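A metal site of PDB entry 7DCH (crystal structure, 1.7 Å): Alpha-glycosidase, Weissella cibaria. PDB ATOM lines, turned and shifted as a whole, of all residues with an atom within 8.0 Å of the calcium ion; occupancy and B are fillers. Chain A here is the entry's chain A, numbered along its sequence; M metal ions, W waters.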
ATOM      1  N   PRO A 150      -6.220  12.514  -1.907  1.00  0.00           N
ATOM      2  CA  PRO A 150      -5.582  13.475  -0.975  1.00  0.00           C
ATOM      3  C   PRO A 150      -4.382  12.921  -0.215  1.00  0.00           C
ATOM      4  O   PRO A 150      -3.489  13.700   0.139  1.00  0.00           O
ATOM      5  CB  PRO A 150      -6.720  13.857  -0.017  1.00  0.00           C
ATOM      6  CG  PRO A 150      -7.964  13.376  -0.636  1.00  0.00           C
ATOM      7  CD  PRO A 150      -7.642  12.292  -1.612  1.00  0.00           C
ATOM      8  N   GLU A 151      -4.321  11.623   0.031  1.00  0.00           N
ATOM      9  CA  GLU A 151      -3.164  11.086   0.727  1.00  0.00           C
ATOM     10  C   GLU A 151      -1.877  11.308  -0.063  1.00  0.00           C
ATOM     11  O   GLU A 151      -0.796  11.206   0.526  1.00  0.00           O
ATOM     12  CB  GLU A 151      -3.336   9.584   0.974  1.00  0.00           C
ATOM     13  CG  GLU A 151      -3.034   9.106   2.399  1.00  0.00           C
ATOM     14  CD  GLU A 151      -1.549   8.972   2.687  1.00  0.00           C
ATOM     15  OE1 GLU A 151      -1.145   9.486   3.773  1.00  0.00           O
ATOM     16  OE2 GLU A 151      -0.806   8.350   1.873  1.00  0.00           O
ATOM     17  N   ALA A 154      -0.062  16.384  -1.500  1.00  0.00           N
ATOM     18  CA  ALA A 154       0.968  17.172  -0.837  1.00  0.00           C
ATOM     19  C   ALA A 154       0.789  17.089   0.665  1.00  0.00           C
ATOM     20  O   ALA A 154      -0.330  17.209   1.171  1.00  0.00           O
ATOM     21  CB  ALA A 154       0.934  18.618  -1.320  1.00  0.00           C
ATOM     22  N   ASN A 155       1.887  16.861   1.380  1.00  0.00           N
ATOM     23  CA  ASN A 155       1.903  16.852   2.831  1.00  0.00           C
ATOM     24  C   ASN A 155       2.189  18.276   3.302  1.00  0.00           C
ATOM     25  O   ASN A 155       3.349  18.718   3.327  1.00  0.00           O
ATOM     26  CB  ASN A 155       2.962  15.865   3.345  1.00  0.00           C
ATOM     27  CG  ASN A 155       2.930  15.706   4.879  1.00  0.00           C
ATOM     28  OD1 ASN A 155       2.090  16.288   5.566  1.00  0.00           O
ATOM     29  ND2 ASN A 155       3.834  14.876   5.400  1.00  0.00           N
ATOM     30  N   GLY A 156       1.150  18.986   3.722  1.00  0.00           N
ATOM     31  CA  GLY A 156       1.288  20.330   4.224  1.00  0.00           C
ATOM     32  C   GLY A 156       1.468  20.426   5.715  1.00  0.00           C
ATOM     33  O   GLY A 156       1.605  21.517   6.255  1.00  0.00           O
ATOM     34  N   ASP A 157       1.461  19.284   6.413  1.00  0.00           N
ATOM     35  CA  ASP A 157       1.506  19.280   7.875  1.00  0.00           C
ATOM     36  C   ASP A 157       1.995  17.911   8.319  1.00  0.00           C
ATOM     37  O   ASP A 157       1.216  16.950   8.350  1.00  0.00           O
ATOM     38  CB  ASP A 157       0.132  19.606   8.439  1.00  0.00           C
ATOM     39  CG  ASP A 157       0.123  19.783   9.941  1.00  0.00           C
ATOM     40  OD1 ASP A 157       1.143  19.457  10.615  1.00  0.00           O
ATOM     41  OD2 ASP A 157      -0.928  20.224  10.469  1.00  0.00           O
ATOM     42  N   VAL A 158       3.276  17.821   8.688  1.00  0.00           N
ATOM     43  CA  VAL A 158       3.787  16.547   9.187  1.00  0.00           C
ATOM     44  C   VAL A 158       3.122  16.145  10.503  1.00  0.00           C
ATOM     45  O   VAL A 158       3.132  14.959  10.852  1.00  0.00           O
ATOM     46  CB  VAL A 158       5.329  16.552   9.389  1.00  0.00           C
ATOM     47  CG1 VAL A 158       6.060  16.690   8.052  1.00  0.00           C
ATOM     48  CG2 VAL A 158       5.771  17.632  10.378  1.00  0.00           C
ATOM     49  N   SER A 159       2.557  17.095  11.255  1.00  0.00           N
ATOM     50  CA  SER A 159       2.098  16.794  12.612  1.00  0.00           C
ATOM     51  C   SER A 159       0.844  15.920  12.627  1.00  0.00           C
ATOM     52  O   SER A 159       0.523  15.359  13.673  1.00  0.00           O
ATOM     53  CB  SER A 159       1.843  18.090  13.400  1.00  0.00           C
ATOM     54  OG  SER A 159       0.637  18.730  13.018  1.00  0.00           O
ATOM     55  N   ASN A 160       0.135  15.775  11.498  1.00  0.00           N
ATOM     56  CA  ASN A 160      -1.029  14.899  11.452  1.00  0.00           C
ATOM     57  C   ASN A 160      -0.734  13.592  10.742  1.00  0.00           C
ATOM     58  O   ASN A 160      -1.664  12.845  10.421  1.00  0.00           O
ATOM     59  CB  ASN A 160      -2.209  15.616  10.795  1.00  0.00           C
ATOM     60  CG  ASN A 160      -1.911  16.059   9.346  1.00  0.00           C
ATOM     61  OD1 ASN A 160      -1.027  15.521   8.680  1.00  0.00           O
ATOM     62  ND2 ASN A 160      -2.667  17.061   8.886  1.00  0.00           N
ATOM     63  N   ASP A 161       0.533  13.275  10.492  1.00  0.00           N
ATOM     64  CA  ASP A 161       0.855  12.114   9.656  1.00  0.00           C
ATOM     65  C   ASP A 161       0.482  10.824  10.374  1.00  0.00           C
ATOM     66  O   ASP A 161       0.651  10.707  11.588  1.00  0.00           O
ATOM     67  CB  ASP A 161       2.344  12.085   9.277  1.00  0.00           C
ATOM     68  CG  ASP A 161       2.710  13.120   8.201  1.00  0.00           C
ATOM     69  OD1 ASP A 161       1.795  13.743   7.631  1.00  0.00           O
ATOM     70  OD2 ASP A 161       3.907  13.299   7.936  1.00  0.00           O
ATOM     71  N   PRO A 162      -0.049   9.838   9.649  1.00  0.00           N
ATOM     72  CA  PRO A 162      -0.241   8.500  10.220  1.00  0.00           C
ATOM     73  C   PRO A 162       1.075   7.902  10.723  1.00  0.00           C
ATOM     74  O   PRO A 162       2.170   8.261  10.290  1.00  0.00           O
ATOM     75  CB  PRO A 162      -0.804   7.689   9.034  1.00  0.00           C
ATOM     76  CG  PRO A 162      -1.401   8.740   8.107  1.00  0.00           C
ATOM     77  CD  PRO A 162      -0.466   9.906   8.241  1.00  0.00           C
ATOM     78  N   THR A 165       4.361   6.762   8.390  1.00  0.00           N
ATOM     79  CA  THR A 165       4.434   7.559   7.168  1.00  0.00           C
ATOM     80  C   THR A 165       5.823   7.472   6.543  1.00  0.00           C
ATOM     81  O   THR A 165       6.841   7.539   7.230  1.00  0.00           O
ATOM     82  CB  THR A 165       4.032   9.018   7.485  1.00  0.00           C
ATOM     83  OG1 THR A 165       2.632   9.048   7.850  1.00  0.00           O
ATOM     84  CG2 THR A 165       4.280   9.948   6.284  1.00  0.00           C
ATOM     85  N   TRP A 168       8.486  11.290   1.335  1.00  0.00           N
ATOM     86  CA  TRP A 168       7.769  11.618   0.103  1.00  0.00           C
ATOM     87  C   TRP A 168       8.657  11.338  -1.104  1.00  0.00           C
ATOM     88  O   TRP A 168       9.755  11.898  -1.202  1.00  0.00           O
ATOM     89  CB  TRP A 168       7.336  13.081   0.118  1.00  0.00           C
ATOM     90  CG  TRP A 168       6.293  13.402  -0.891  1.00  0.00           C
ATOM     91  CD1 TRP A 168       6.487  13.691  -2.208  1.00  0.00           C
ATOM     92  CD2 TRP A 168       4.878  13.479  -0.670  1.00  0.00           C
ATOM     93  NE1 TRP A 168       5.282  13.950  -2.824  1.00  0.00           N
ATOM     94  CE2 TRP A 168       4.279  13.822  -1.902  1.00  0.00           C
ATOM     95  CE3 TRP A 168       4.053  13.304   0.452  1.00  0.00           C
ATOM     96  CZ2 TRP A 168       2.886  13.998  -2.041  1.00  0.00           C
ATOM     97  CZ3 TRP A 168       2.693  13.443   0.322  1.00  0.00           C
ATOM     98  CH2 TRP A 168       2.103  13.795  -0.936  1.00  0.00           C
ATOM     99  N   TYR A 180       1.799   8.325   3.000  1.00  0.00           N
ATOM    100  CA  TYR A 180       2.800   9.340   2.695  1.00  0.00           C
ATOM    101  C   TYR A 180       2.482  10.692   3.325  1.00  0.00           C
ATOM    102  O   TYR A 180       3.328  11.610   3.255  1.00  0.00           O
ATOM    103  CB  TYR A 180       2.943   9.497   1.175  1.00  0.00           C
ATOM    104  CG  TYR A 180       3.639   8.322   0.538  1.00  0.00           C
ATOM    105  CD1 TYR A 180       2.908   7.218   0.083  1.00  0.00           C
ATOM    106  CD2 TYR A 180       5.012   8.300   0.426  1.00  0.00           C
ATOM    107  CE1 TYR A 180       3.559   6.137  -0.488  1.00  0.00           C
ATOM    108  CE2 TYR A 180       5.664   7.217  -0.111  1.00  0.00           C
ATOM    109  CZ  TYR A 180       4.941   6.148  -0.574  1.00  0.00           C
ATOM    110  OH  TYR A 180       5.593   5.086  -1.137  1.00  0.00           O
ATOM    111  N   GLY A 181       1.340  10.843   3.969  1.00  0.00           N
ATOM    112  CA  GLY A 181       1.075  12.027   4.767  1.00  0.00           C
ATOM    113  C   GLY A 181       0.354  13.139   4.057  1.00  0.00           C
ATOM    114  O   GLY A 181       0.229  14.231   4.632  1.00  0.00           O
ATOM    115  N   GLY A 182      -0.172  12.904   2.856  1.00  0.00           N
ATOM    116  CA  GLY A 182      -0.879  13.962   2.141  1.00  0.00           C
ATOM    117  C   GLY A 182      -2.088  14.441   2.921  1.00  0.00           C
ATOM    118  O   GLY A 182      -2.683  13.688   3.701  1.00  0.00           O
ATOM    119  N   ASP A 183      -2.445  15.715   2.778  1.00  0.00           N
ATOM    120  CA  ASP A 183      -3.498  16.251   3.634  1.00  0.00           C
ATOM    121  C   ASP A 183      -4.121  17.500   2.997  1.00  0.00           C
ATOM    122  O   ASP A 183      -3.716  17.958   1.928  1.00  0.00           O
ATOM    123  CB  ASP A 183      -2.938  16.531   5.042  1.00  0.00           C
ATOM    124  CG  ASP A 183      -1.672  17.406   5.022  1.00  0.00           C
ATOM    125  OD1 ASP A 183      -1.597  18.374   4.236  1.00  0.00           O
ATOM    126  OD2 ASP A 183      -0.750  17.143   5.820  1.00  0.00           O
ATOM    127  N   LEU A 184      -5.124  18.048   3.683  1.00  0.00           N
ATOM    128  CA  LEU A 184      -5.823  19.232   3.165  1.00  0.00           C
ATOM    129  C   LEU A 184      -4.914  20.441   3.115  1.00  0.00           C
ATOM    130  O   LEU A 184      -5.044  21.288   2.202  1.00  0.00           O
ATOM    131  CB  LEU A 184      -7.066  19.558   4.010  1.00  0.00           C
ATOM    132  CG  LEU A 184      -8.177  18.546   3.998  1.00  0.00           C
ATOM    133  CD1 LEU A 184      -9.397  19.123   4.722  1.00  0.00           C
ATOM    134  CD2 LEU A 184      -8.539  18.177   2.543  1.00  0.00           C
ATOM    135  N   GLN A 185      -4.015  20.601   4.100  1.00  0.00           N
ATOM    136  CA  GLN A 185      -3.127  21.746   4.053  1.00  0.00           C
ATOM    137  C   GLN A 185      -2.252  21.708   2.810  1.00  0.00           C
ATOM    138  O   GLN A 185      -1.958  22.754   2.230  1.00  0.00           O
ATOM    139  CB  GLN A 185      -2.268  21.827   5.321  1.00  0.00           C
ATOM    140  CG  GLN A 185      -1.392  23.115   5.402  1.00  0.00           C
ATOM    141  CD  GLN A 185      -2.190  24.436   5.474  1.00  0.00           C
ATOM    142  OE1 GLN A 185      -3.089  24.587   6.303  1.00  0.00           O
ATOM    143  NE2 GLN A 185      -1.879  25.379   4.580  1.00  0.00           N
ATOM    144  N   GLY A 186      -1.863  20.510   2.352  1.00  0.00           N
ATOM    145  CA  GLY A 186      -1.045  20.431   1.141  1.00  0.00           C
ATOM    146  C   GLY A 186      -1.800  20.911  -0.090  1.00  0.00           C
ATOM    147  O   GLY A 186      -1.221  21.534  -1.003  1.00  0.00           O
ATOM    148  N   PRO A 226      -8.891  12.960  10.659  1.00  0.00           N
ATOM    149  CA  PRO A 226      -7.956  13.838  11.380  1.00  0.00           C
ATOM    150  C   PRO A 226      -6.554  13.849  10.806  1.00  0.00           C
ATOM    151  O   PRO A 226      -5.811  14.808  11.054  1.00  0.00           O
ATOM    152  CB  PRO A 226      -7.985  13.304  12.829  1.00  0.00           C
ATOM    153  CG  PRO A 226      -8.827  12.083  12.818  1.00  0.00           C
ATOM    154  CD  PRO A 226      -9.647  12.054  11.550  1.00  0.00           C
ATOM    155  N   HIS A 227      -6.164  12.830  10.036  1.00  0.00           N
ATOM    156  CA  HIS A 227      -4.874  12.886   9.363  1.00  0.00           C
ATOM    157  C   HIS A 227      -4.900  13.802   8.153  1.00  0.00           C
ATOM    158  O   HIS A 227      -3.837  14.144   7.635  1.00  0.00           O
ATOM    159  CB  HIS A 227      -4.461  11.473   8.956  1.00  0.00           C
ATOM    160  CG  HIS A 227      -4.456  10.492  10.089  1.00  0.00           C
ATOM    161  ND1 HIS A 227      -5.509   9.633  10.335  1.00  0.00           N
ATOM    162  CD2 HIS A 227      -3.546  10.257  11.063  1.00  0.00           C
ATOM    163  CE1 HIS A 227      -5.244   8.919  11.411  1.00  0.00           C
ATOM    164  NE2 HIS A 227      -4.061   9.273  11.871  1.00  0.00           N
ATOM    165  N   PHE A 228      -6.081  14.195   7.686  1.00  0.00           N
ATOM    166  CA  PHE A 228      -6.211  15.177   6.622  1.00  0.00           C
ATOM    167  C   PHE A 228      -6.450  16.596   7.125  1.00  0.00           C
ATOM    168  O   PHE A 228      -6.046  17.559   6.439  1.00  0.00           O
ATOM    169  CB  PHE A 228      -7.388  14.827   5.694  1.00  0.00           C
ATOM    170  CG  PHE A 228      -7.120  13.669   4.750  1.00  0.00           C
ATOM    171  CD1 PHE A 228      -5.850  13.155   4.562  1.00  0.00           C
ATOM    172  CD2 PHE A 228      -8.186  13.082   4.073  1.00  0.00           C
ATOM    173  CE1 PHE A 228      -5.630  12.060   3.681  1.00  0.00           C
ATOM    174  CE2 PHE A 228      -7.974  12.017   3.201  1.00  0.00           C
ATOM    175  CZ  PHE A 228      -6.701  11.507   3.004  1.00  0.00           C
ATOM    176  N   GLY A 229      -7.142  16.770   8.246  1.00  0.00           N
ATOM    177  CA  GLY A 229      -7.472  18.120   8.692  1.00  0.00           C
ATOM    178  C   GLY A 229      -8.673  18.092   9.631  1.00  0.00           C
ATOM    179  O   GLY A 229      -8.932  17.102  10.311  1.00  0.00           O
HETATM  180 CA    CA M   1       0.290  15.312   6.804  1.00  0.00          CA
HETATM  181  O   HOH W   1      -1.322  13.475   6.959  1.00  0.00           O
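The side-chain amide nitrogen of Asn 160 sits close to the backbone carbonyl oxygen of His 227 (3.4 Å).
OD1 of Asp 183 lies within hydrogen-bond range of N of Gly 156 (2.9 Å).
The backbone NH of Asp 183 is in hydrogen-bond range of the backbone carbonyl oxygen of Ala 154.
OD1 of Asp 183 lies within hydrogen-bond range of N of Gln 185 (3.3 Å).
The side-chain carboxylate of Asp 183 lies within hydrogen-bond range of the backbone NH of Gly 186.
The backbone NH (N) of Asp 183 lies within hydrogen-bond range of the backbone carbonyl oxygen (O) of Pro 150 (3.5 Å).
OE1 of Glu 151 sits at hydrogen-bond distance from N of Gly 181 (2.8 Å).
The side-chain hydroxyl (OG) of Ser 159 is in hydrogen-bond range of the side-chain carboxylate (OD1) of Asp 157 (2.6 Å).
The nearest printed residue that does not touch the calcium ion is Val 158 (4.3 Å).
The calcium ion is bound by the side-chain amide oxygen of Asn 160 (2.3 Å), the side-chain carboxylate of Asp 183 (2.3 Å), the side-chain carboxylate of Asp 161 (2.3 Å), the side-chain amide oxygen of Asn 155 (2.4 Å), the backbone carbonyl oxygen of Gly 181 (2.4 Å), the backbone carbonyl oxygen of Asp 157 (2.4 Å) and water W1 (2.4 Å).
The calcium ion has seven donor atoms within binding distance.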
